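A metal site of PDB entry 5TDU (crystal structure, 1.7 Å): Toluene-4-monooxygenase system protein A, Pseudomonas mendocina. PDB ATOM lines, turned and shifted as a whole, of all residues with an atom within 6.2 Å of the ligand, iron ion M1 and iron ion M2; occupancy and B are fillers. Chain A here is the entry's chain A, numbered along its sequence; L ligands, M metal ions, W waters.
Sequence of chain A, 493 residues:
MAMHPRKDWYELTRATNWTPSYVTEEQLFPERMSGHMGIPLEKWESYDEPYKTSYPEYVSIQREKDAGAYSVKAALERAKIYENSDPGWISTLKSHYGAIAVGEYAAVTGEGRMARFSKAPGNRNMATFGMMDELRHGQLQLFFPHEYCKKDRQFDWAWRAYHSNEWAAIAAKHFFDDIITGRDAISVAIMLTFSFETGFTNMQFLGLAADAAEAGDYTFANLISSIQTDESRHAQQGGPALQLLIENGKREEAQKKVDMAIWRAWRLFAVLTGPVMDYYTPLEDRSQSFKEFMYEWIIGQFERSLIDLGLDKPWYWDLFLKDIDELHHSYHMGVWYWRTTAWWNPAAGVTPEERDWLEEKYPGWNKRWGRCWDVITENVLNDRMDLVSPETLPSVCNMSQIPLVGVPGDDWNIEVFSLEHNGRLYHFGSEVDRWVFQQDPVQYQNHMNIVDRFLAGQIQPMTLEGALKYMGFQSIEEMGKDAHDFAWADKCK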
ATOM      1  N   ALA A  99      -1.609 -23.712  14.632  1.00  0.00           N
ATOM      2  CA  ALA A  99      -2.893 -23.341  15.220  1.00  0.00           C
ATOM      3  C   ALA A  99      -2.990 -21.850  15.487  1.00  0.00           C
ATOM      4  O   ALA A  99      -4.083 -21.316  15.640  1.00  0.00           O
ATOM      5  CB  ALA A  99      -3.120 -24.121  16.488  1.00  0.00           C
ATOM      6  N   ILE A 100      -1.856 -21.156  15.482  1.00  0.00           N
ATOM      7  CA  ILE A 100      -1.801 -19.774  15.972  1.00  0.00           C
ATOM      8  C   ILE A 100      -1.445 -18.729  14.915  1.00  0.00           C
ATOM      9  O   ILE A 100      -2.038 -17.652  14.861  1.00  0.00           O
ATOM     10  CB  ILE A 100      -0.803 -19.681  17.157  1.00  0.00           C
ATOM     11  CG1 ILE A 100      -1.340 -20.446  18.375  1.00  0.00           C
ATOM     12  CG2 ILE A 100      -0.495 -18.228  17.497  1.00  0.00           C
ATOM     13  CD1 ILE A 100      -2.609 -19.852  18.988  1.00  0.00           C
ATOM     14  N   GLY A 103      -4.139 -17.280  12.655  1.00  0.00           N
ATOM     15  CA  GLY A 103      -5.172 -16.765  13.552  1.00  0.00           C
ATOM     16  C   GLY A 103      -4.778 -15.411  14.141  1.00  0.00           C
ATOM     17  O   GLY A 103      -5.626 -14.517  14.320  1.00  0.00           O
ATOM     18  N   GLU A 104      -3.500 -15.258  14.465  1.00  0.00           N
ATOM     19  CA  GLU A 104      -2.976 -13.947  14.866  1.00  0.00           C
ATOM     20  C   GLU A 104      -3.268 -12.915  13.782  1.00  0.00           C
ATOM     21  O   GLU A 104      -3.687 -11.796  14.051  1.00  0.00           O
ATOM     22  CB  GLU A 104      -1.472 -13.998  15.120  1.00  0.00           C
ATOM     23  CG  GLU A 104      -1.057 -14.899  16.261  1.00  0.00           C
ATOM     24  CD  GLU A 104      -0.874 -14.151  17.564  1.00  0.00           C
ATOM     25  OE1 GLU A 104      -0.124 -14.639  18.428  1.00  0.00           O
ATOM     26  OE2 GLU A 104      -1.482 -13.073  17.718  1.00  0.00           O
ATOM     27  N   TYR A 105      -2.982 -13.282  12.543  1.00  0.00           N
ATOM     28  CA  TYR A 105      -3.218 -12.363  11.445  1.00  0.00           C
ATOM     29  C   TYR A 105      -4.716 -12.064  11.336  1.00  0.00           C
ATOM     30  O   TYR A 105      -5.102 -10.927  11.017  1.00  0.00           O
ATOM     31  CB  TYR A 105      -2.670 -12.904  10.114  1.00  0.00           C
ATOM     32  CG  TYR A 105      -2.800 -11.862   9.025  1.00  0.00           C
ATOM     33  CD1 TYR A 105      -1.958 -10.752   9.022  1.00  0.00           C
ATOM     34  CD2 TYR A 105      -3.781 -11.961   8.044  1.00  0.00           C
ATOM     35  CE1 TYR A 105      -2.092  -9.779   8.050  1.00  0.00           C
ATOM     36  CE2 TYR A 105      -3.905 -10.997   7.070  1.00  0.00           C
ATOM     37  CZ  TYR A 105      -3.064  -9.903   7.087  1.00  0.00           C
ATOM     38  OH  TYR A 105      -3.193  -8.926   6.123  1.00  0.00           O
ATOM     39  N   ALA A 107      -6.615 -11.830  13.809  1.00  0.00           N
ATOM     40  CA  ALA A 107      -6.937 -10.922  14.901  1.00  0.00           C
ATOM     41  C   ALA A 107      -6.755  -9.457  14.505  1.00  0.00           C
ATOM     42  O   ALA A 107      -7.341  -8.567  15.121  1.00  0.00           O
ATOM     43  CB  ALA A 107      -6.092 -11.256  16.142  1.00  0.00           C
ATOM     44  N   GLU A 111      -9.336  -6.290  15.616  1.00  0.00           N
ATOM     45  CA  GLU A 111      -8.860  -4.989  16.038  1.00  0.00           C
ATOM     46  C   GLU A 111      -9.331  -3.922  15.039  1.00  0.00           C
ATOM     47  O   GLU A 111      -9.770  -2.840  15.435  1.00  0.00           O
ATOM     48  CB  GLU A 111      -7.328  -4.994  16.156  1.00  0.00           C
ATOM     49  CG  GLU A 111      -6.797  -5.865  17.313  1.00  0.00           C
ATOM     50  CD  GLU A 111      -7.026  -5.251  18.702  1.00  0.00           C
ATOM     51  OE1 GLU A 111      -7.386  -4.071  18.772  1.00  0.00           O
ATOM     52  OE2 GLU A 111      -6.816  -5.956  19.717  1.00  0.00           O
ATOM     53  N   ASP A 133      -0.052  -4.693  16.456  1.00  0.00           N
ATOM     54  CA  ASP A 133       0.450  -5.792  17.274  1.00  0.00           C
ATOM     55  C   ASP A 133       0.177  -7.136  16.631  1.00  0.00           C
ATOM     56  O   ASP A 133       1.034  -8.012  16.602  1.00  0.00           O
ATOM     57  CB  ASP A 133      -0.195  -5.815  18.671  1.00  0.00           C
ATOM     58  CG  ASP A 133       0.205  -4.635  19.538  1.00  0.00           C
ATOM     59  OD1 ASP A 133       1.253  -3.981  19.280  1.00  0.00           O
ATOM     60  OD2 ASP A 133      -0.531  -4.385  20.506  1.00  0.00           O
ATOM     61  N   GLU A 134      -1.060  -7.348  16.168  1.00  0.00           N
ATOM     62  CA  GLU A 134      -1.414  -8.660  15.661  1.00  0.00           C
ATOM     63  C   GLU A 134      -0.710  -8.915  14.329  1.00  0.00           C
ATOM     64  O   GLU A 134      -0.391 -10.049  13.991  1.00  0.00           O
ATOM     65  CB  GLU A 134      -2.929  -8.802  15.505  1.00  0.00           C
ATOM     66  CG  GLU A 134      -3.735  -8.591  16.807  1.00  0.00           C
ATOM     67  CD  GLU A 134      -3.395  -9.573  17.928  1.00  0.00           C
ATOM     68  OE1 GLU A 134      -2.390 -10.321  17.841  1.00  0.00           O
ATOM     69  OE2 GLU A 134      -4.163  -9.609  18.907  1.00  0.00           O
ATOM     70  N   HIS A 137       2.505 -10.240  15.328  1.00  0.00           N
ATOM     71  CA  HIS A 137       2.403 -11.603  15.845  1.00  0.00           C
ATOM     72  C   HIS A 137       2.228 -12.602  14.714  1.00  0.00           C
ATOM     73  O   HIS A 137       2.811 -13.685  14.752  1.00  0.00           O
ATOM     74  CB  HIS A 137       1.241 -11.710  16.837  1.00  0.00           C
ATOM     75  CG  HIS A 137       1.408 -10.800  18.022  1.00  0.00           C
ATOM     76  ND1 HIS A 137       0.423 -10.611  18.971  1.00  0.00           N
ATOM     77  CD2 HIS A 137       2.450 -10.017  18.401  1.00  0.00           C
ATOM     78  CE1 HIS A 137       0.849  -9.759  19.893  1.00  0.00           C
ATOM     79  NE2 HIS A 137       2.086  -9.377  19.564  1.00  0.00           N
ATOM     80  N   GLN A 141       5.245 -15.339  13.667  1.00  0.00           N
ATOM     81  CA  GLN A 141       4.976 -16.752  13.835  1.00  0.00           C
ATOM     82  C   GLN A 141       4.833 -17.474  12.497  1.00  0.00           C
ATOM     83  O   GLN A 141       4.608 -18.680  12.466  1.00  0.00           O
ATOM     84  CB  GLN A 141       3.767 -16.927  14.735  1.00  0.00           C
ATOM     85  CG  GLN A 141       4.179 -16.669  16.193  1.00  0.00           C
ATOM     86  CD  GLN A 141       3.028 -16.590  17.165  1.00  0.00           C
ATOM     87  OE1 GLN A 141       2.953 -17.370  18.102  1.00  0.00           O
ATOM     88  NE2 GLN A 141       2.145 -15.616  16.948  1.00  0.00           N
ATOM     89  N   TYR A 162      -4.795 -22.888   8.346  1.00  0.00           N
ATOM     90  CA  TYR A 162      -6.058 -22.138   8.256  1.00  0.00           C
ATOM     91  C   TYR A 162      -6.635 -22.148   6.851  1.00  0.00           C
ATOM     92  O   TYR A 162      -7.789 -21.778   6.647  1.00  0.00           O
ATOM     93  CB  TYR A 162      -5.872 -20.692   8.725  1.00  0.00           C
ATOM     94  CG  TYR A 162      -5.916 -20.524  10.230  1.00  0.00           C
ATOM     95  CD1 TYR A 162      -4.979 -21.134  11.065  1.00  0.00           C
ATOM     96  CD2 TYR A 162      -6.896 -19.729  10.819  1.00  0.00           C
ATOM     97  CE1 TYR A 162      -5.032 -20.967  12.438  1.00  0.00           C
ATOM     98  CE2 TYR A 162      -6.945 -19.549  12.197  1.00  0.00           C
ATOM     99  CZ  TYR A 162      -6.007 -20.170  12.998  1.00  0.00           C
ATOM    100  OH  TYR A 162      -6.045 -19.985  14.355  1.00  0.00           O
ATOM    101  N   PHE A 176     -12.249 -18.645  16.310  1.00  0.00           N
ATOM    102  CA  PHE A 176     -11.738 -17.304  16.046  1.00  0.00           C
ATOM    103  C   PHE A 176     -12.677 -16.512  15.151  1.00  0.00           C
ATOM    104  O   PHE A 176     -12.828 -15.295  15.313  1.00  0.00           O
ATOM    105  CB  PHE A 176     -10.327 -17.386  15.448  1.00  0.00           C
ATOM    106  CG  PHE A 176      -9.311 -17.829  16.440  1.00  0.00           C
ATOM    107  CD1 PHE A 176      -9.238 -17.208  17.689  1.00  0.00           C
ATOM    108  CD2 PHE A 176      -8.456 -18.878  16.170  1.00  0.00           C
ATOM    109  CE1 PHE A 176      -8.321 -17.618  18.629  1.00  0.00           C
ATOM    110  CE2 PHE A 176      -7.530 -19.288  17.105  1.00  0.00           C
ATOM    111  CZ  PHE A 176      -7.468 -18.674  18.338  1.00  0.00           C
ATOM    112  N   ILE A 180     -13.601 -13.274  16.933  1.00  0.00           N
ATOM    113  CA  ILE A 180     -12.710 -12.227  16.414  1.00  0.00           C
ATOM    114  C   ILE A 180     -13.276 -11.535  15.177  1.00  0.00           C
ATOM    115  O   ILE A 180     -13.410 -10.322  15.155  1.00  0.00           O
ATOM    116  CB  ILE A 180     -11.321 -12.791  16.075  1.00  0.00           C
ATOM    117  CG1 ILE A 180     -10.680 -13.428  17.317  1.00  0.00           C
ATOM    118  CG2 ILE A 180     -10.431 -11.695  15.474  1.00  0.00           C
ATOM    119  CD1 ILE A 180      -9.216 -13.803  17.104  1.00  0.00           C
ATOM    120  N   LEU A 192     -12.897 -11.116  22.586  1.00  0.00           N
ATOM    121  CA  LEU A 192     -11.483 -11.230  22.249  1.00  0.00           C
ATOM    122  C   LEU A 192     -10.588 -10.554  23.286  1.00  0.00           C
ATOM    123  O   LEU A 192      -9.819 -11.236  23.967  1.00  0.00           O
ATOM    124  CB  LEU A 192     -11.208 -10.640  20.865  1.00  0.00           C
ATOM    125  CG  LEU A 192      -9.724 -10.546  20.488  1.00  0.00           C
ATOM    126  CD1 LEU A 192      -9.075 -11.933  20.508  1.00  0.00           C
ATOM    127  CD2 LEU A 192      -9.582  -9.887  19.110  1.00  0.00           C
ATOM    128  N   PHE A 196     -10.606 -13.661  25.928  1.00  0.00           N
ATOM    129  CA  PHE A 196      -9.568 -14.529  25.383  1.00  0.00           C
ATOM    130  C   PHE A 196      -8.165 -14.035  25.728  1.00  0.00           C
ATOM    131  O   PHE A 196      -7.312 -14.804  26.169  1.00  0.00           O
ATOM    132  CB  PHE A 196      -9.736 -14.664  23.873  1.00  0.00           C
ATOM    133  CG  PHE A 196      -8.757 -15.597  23.216  1.00  0.00           C
ATOM    134  CD1 PHE A 196      -8.761 -16.955  23.508  1.00  0.00           C
ATOM    135  CD2 PHE A 196      -7.833 -15.113  22.281  1.00  0.00           C
ATOM    136  CE1 PHE A 196      -7.857 -17.821  22.896  1.00  0.00           C
ATOM    137  CE2 PHE A 196      -6.943 -15.971  21.663  1.00  0.00           C
ATOM    138  CZ  PHE A 196      -6.951 -17.326  21.968  1.00  0.00           C
ATOM    139  N   GLU A 197      -7.937 -12.729  25.542  1.00  0.00           N
ATOM    140  CA  GLU A 197      -6.576 -12.179  25.618  1.00  0.00           C
ATOM    141  C   GLU A 197      -6.091 -11.798  27.030  1.00  0.00           C
ATOM    142  O   GLU A 197      -4.880 -11.669  27.245  1.00  0.00           O
ATOM    143  CB  GLU A 197      -6.479 -10.946  24.696  1.00  0.00           C
ATOM    144  CG  GLU A 197      -6.565 -11.311  23.227  1.00  0.00           C
ATOM    145  CD  GLU A 197      -6.401 -10.113  22.302  1.00  0.00           C
ATOM    146  OE1 GLU A 197      -6.883  -9.011  22.643  1.00  0.00           O
ATOM    147  OE2 GLU A 197      -5.776 -10.261  21.237  1.00  0.00           O
ATOM    148  N   THR A 201      -4.877 -16.709  26.681  1.00  0.00           N
ATOM    149  CA  THR A 201      -3.637 -16.743  25.909  1.00  0.00           C
ATOM    150  C   THR A 201      -2.401 -16.836  26.808  1.00  0.00           C
ATOM    151  O   THR A 201      -1.359 -17.330  26.371  1.00  0.00           O
ATOM    152  CB  THR A 201      -3.481 -15.529  24.970  1.00  0.00           C
ATOM    153  OG1 THR A 201      -3.571 -14.317  25.720  1.00  0.00           O
ATOM    154  CG2 THR A 201      -4.582 -15.540  23.917  1.00  0.00           C
ATOM    155  N   PHE A 205       1.120 -18.744  25.785  1.00  0.00           N
ATOM    156  CA  PHE A 205       2.246 -17.866  25.499  1.00  0.00           C
ATOM    157  C   PHE A 205       3.153 -17.608  26.711  1.00  0.00           C
ATOM    158  O   PHE A 205       4.250 -17.050  26.561  1.00  0.00           O
ATOM    159  CB  PHE A 205       1.759 -16.525  24.935  1.00  0.00           C
ATOM    160  CG  PHE A 205       1.180 -16.622  23.554  1.00  0.00           C
ATOM    161  CD1 PHE A 205      -0.115 -17.068  23.346  1.00  0.00           C
ATOM    162  CD2 PHE A 205       1.945 -16.258  22.443  1.00  0.00           C
ATOM    163  CE1 PHE A 205      -0.644 -17.158  22.067  1.00  0.00           C
ATOM    164  CE2 PHE A 205       1.430 -16.345  21.167  1.00  0.00           C
ATOM    165  CZ  PHE A 205       0.133 -16.797  20.975  1.00  0.00           C
ATOM    166  N   ILE A 227       5.801 -11.604  22.525  1.00  0.00           N
ATOM    167  CA  ILE A 227       4.479 -11.422  21.942  1.00  0.00           C
ATOM    168  C   ILE A 227       3.460 -11.065  23.032  1.00  0.00           C
ATOM    169  O   ILE A 227       2.617 -10.181  22.850  1.00  0.00           O
ATOM    170  CB  ILE A 227       4.064 -12.699  21.174  1.00  0.00           C
ATOM    171  CG1 ILE A 227       4.834 -12.760  19.858  1.00  0.00           C
ATOM    172  CG2 ILE A 227       2.542 -12.713  20.957  1.00  0.00           C
ATOM    173  CD1 ILE A 227       4.651 -14.049  19.049  1.00  0.00           C
ATOM    174  N   ASP A 230       2.803  -7.465  24.175  1.00  0.00           N
ATOM    175  CA  ASP A 230       1.861  -6.676  23.371  1.00  0.00           C
ATOM    176  C   ASP A 230       0.424  -6.980  23.768  1.00  0.00           C
ATOM    177  O   ASP A 230      -0.396  -6.082  23.915  1.00  0.00           O
ATOM    178  CB  ASP A 230       1.999  -6.996  21.882  1.00  0.00           C
ATOM    179  CG  ASP A 230       3.360  -6.651  21.317  1.00  0.00           C
ATOM    180  OD1 ASP A 230       3.990  -5.658  21.768  1.00  0.00           O
ATOM    181  OD2 ASP A 230       3.795  -7.393  20.399  1.00  0.00           O
ATOM    182  N   GLU A 231       0.136  -8.277  23.875  1.00  0.00           N
ATOM    183  CA  GLU A 231      -1.158  -8.765  24.331  1.00  0.00           C
ATOM    184  C   GLU A 231      -1.576  -8.028  25.589  1.00  0.00           C
ATOM    185  O   GLU A 231      -2.727  -7.559  25.730  1.00  0.00           O
ATOM    186  CB  GLU A 231      -1.082 -10.269  24.594  1.00  0.00           C
ATOM    187  CG  GLU A 231      -2.412 -10.909  24.986  1.00  0.00           C
ATOM    188  CD  GLU A 231      -3.197 -11.370  23.781  1.00  0.00           C
ATOM    189  OE1 GLU A 231      -3.588 -12.558  23.745  1.00  0.00           O
ATOM    190  OE2 GLU A 231      -3.414 -10.551  22.860  1.00  0.00           O
ATOM    191  N   HIS A 234      -2.819  -4.422  24.553  1.00  0.00           N
ATOM    192  CA  HIS A 234      -4.058  -4.210  23.794  1.00  0.00           C
ATOM    193  C   HIS A 234      -5.250  -4.994  24.370  1.00  0.00           C
ATOM    194  O   HIS A 234      -6.411  -4.659  24.098  1.00  0.00           O
ATOM    195  CB  HIS A 234      -3.869  -4.491  22.270  1.00  0.00           C
ATOM    196  CG  HIS A 234      -3.564  -5.914  21.896  1.00  0.00           C
ATOM    197  ND1 HIS A 234      -2.436  -6.252  21.181  1.00  0.00           N
ATOM    198  CD2 HIS A 234      -4.275  -7.055  22.042  1.00  0.00           C
ATOM    199  CE1 HIS A 234      -2.443  -7.548  20.938  1.00  0.00           C
ATOM    200  NE2 HIS A 234      -3.552  -8.066  21.453  1.00  0.00           N
ATOM    201  N   ALA A 235      -4.992  -5.996  25.201  1.00  0.00           N
ATOM    202  CA  ALA A 235      -6.095  -6.730  25.862  1.00  0.00           C
ATOM    203  C   ALA A 235      -6.855  -5.817  26.826  1.00  0.00           C
ATOM    204  O   ALA A 235      -8.021  -6.091  27.166  1.00  0.00           O
ATOM    205  CB  ALA A 235      -5.559  -7.978  26.595  1.00  0.00           C
HETATM  206  C1  LIG L   1      -5.086 -17.103  17.823  1.00  0.00           C
HETATM  207  C2  LIG L   1      -4.683 -15.798  18.451  1.00  0.00           C
HETATM  208  C3  LIG L   1      -5.317 -14.685  18.034  1.00  0.00           C
HETATM  209  C4  LIG L   1      -4.981 -13.512  18.545  1.00  0.00           C
HETATM  210  C5  LIG L   1      -3.703 -15.765  19.359  1.00  0.00           C
HETATM  211  C6  LIG L   1      -3.326 -14.567  19.897  1.00  0.00           C
HETATM  212  C7  LIG L   1      -3.972 -13.441  19.457  1.00  0.00           C
HETATM  213  O1  LIG L   1      -3.636 -12.260  19.928  1.00  0.00           O
HETATM  214 FE    FE M   1      -1.484 -11.646  19.234  1.00  0.00          FE
HETATM  215 FE    FE M   2      -3.820 -10.248  20.934  1.00  0.00          FE
HETATM  216  O   HOH W   1      -1.709 -10.393  21.097  1.00  0.00           O
HETATM  217  O   HOH W   2      -0.609 -13.204  20.541  1.00  0.00           O
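Of the 24 residues printed, 3 come within 4 Å of iron ion M1.
The backbone carbonyl oxygen (O) of Glu 197 lies within hydrogen-bond range of the side-chain hydroxyl (OG1) of Thr 201 (3.3 Å).
The backbone NH (N) of Glu 197 is in hydrogen-bond range of the backbone carbonyl oxygen (O) of Leu 192, at 2.9 Å.
The side-chain carboxylate of Glu 104 sits at hydrogen-bond distance from the side-chain amide nitrogen of Gln 141 (2.9 Å).
A ring nitrogen (NE2) of His 137 is in hydrogen-bond range of the backbone carbonyl oxygen of Ile 227 (3.4 Å).
NE2 of His 137 sits at hydrogen-bond distance from OD2 of Asp 230 (2.7 Å).
A ring nitrogen (ND1) of His 234 is in hydrogen-bond range of the side-chain carboxylate (OD2) of Asp 133 (2.8 Å).
A ring nitrogen (ND1) of His 234 is in hydrogen-bond range of the backbone carbonyl oxygen of Asp 230 (3.4 Å).
O of Phe 196 lies within hydrogen-bond range of N of Thr 201 (3.1 Å).
OE2 of Glu 197 is bound to iron ion M2, 2.0 Å away.
The side-chain carboxylate (OE2) of Glu 231 is bound to iron ion M2 (2.0 Å).
Water W1 binds iron ion M2 (2.1 Å).
Iron ion M2 is bound by the side-chain carboxylate (OE2) of Glu 134 (2.2 Å).
Iron ion M2 is bound by O1 of the ligand (2.3 Å).
NE2 of His 234 binds iron ion M2, at 2.3 Å.
Ile 100 touches the ligand.
Gly 103 touches the ligand.
Ala 107 touches the ligand (CB to C4, 3.5 Å).
CZ of Phe 176 touches C1 of the ligand (2.9 Å).
Phe 196 touches the ligand (CE2 to C2, 3.9 Å).
Within 4 Å of the ligand: Ile 100, Gly 103, Glu 104, Ala 107, Glu 134, Phe 176, Phe 196, Glu 197 and Glu 231.
The nearest printed residue that does not touch the ligand is Ile 180 (4.1 Å).
Iron ion M1 is bound by OE2 of Glu 104 (2.1 Å), OE1 of Glu 134 (2.1 Å), ND1 of His 137 (2.2 Å), water W2 (2.2 Å), water W1 (2.3 Å) and O1 of the ligand (2.3 Å).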
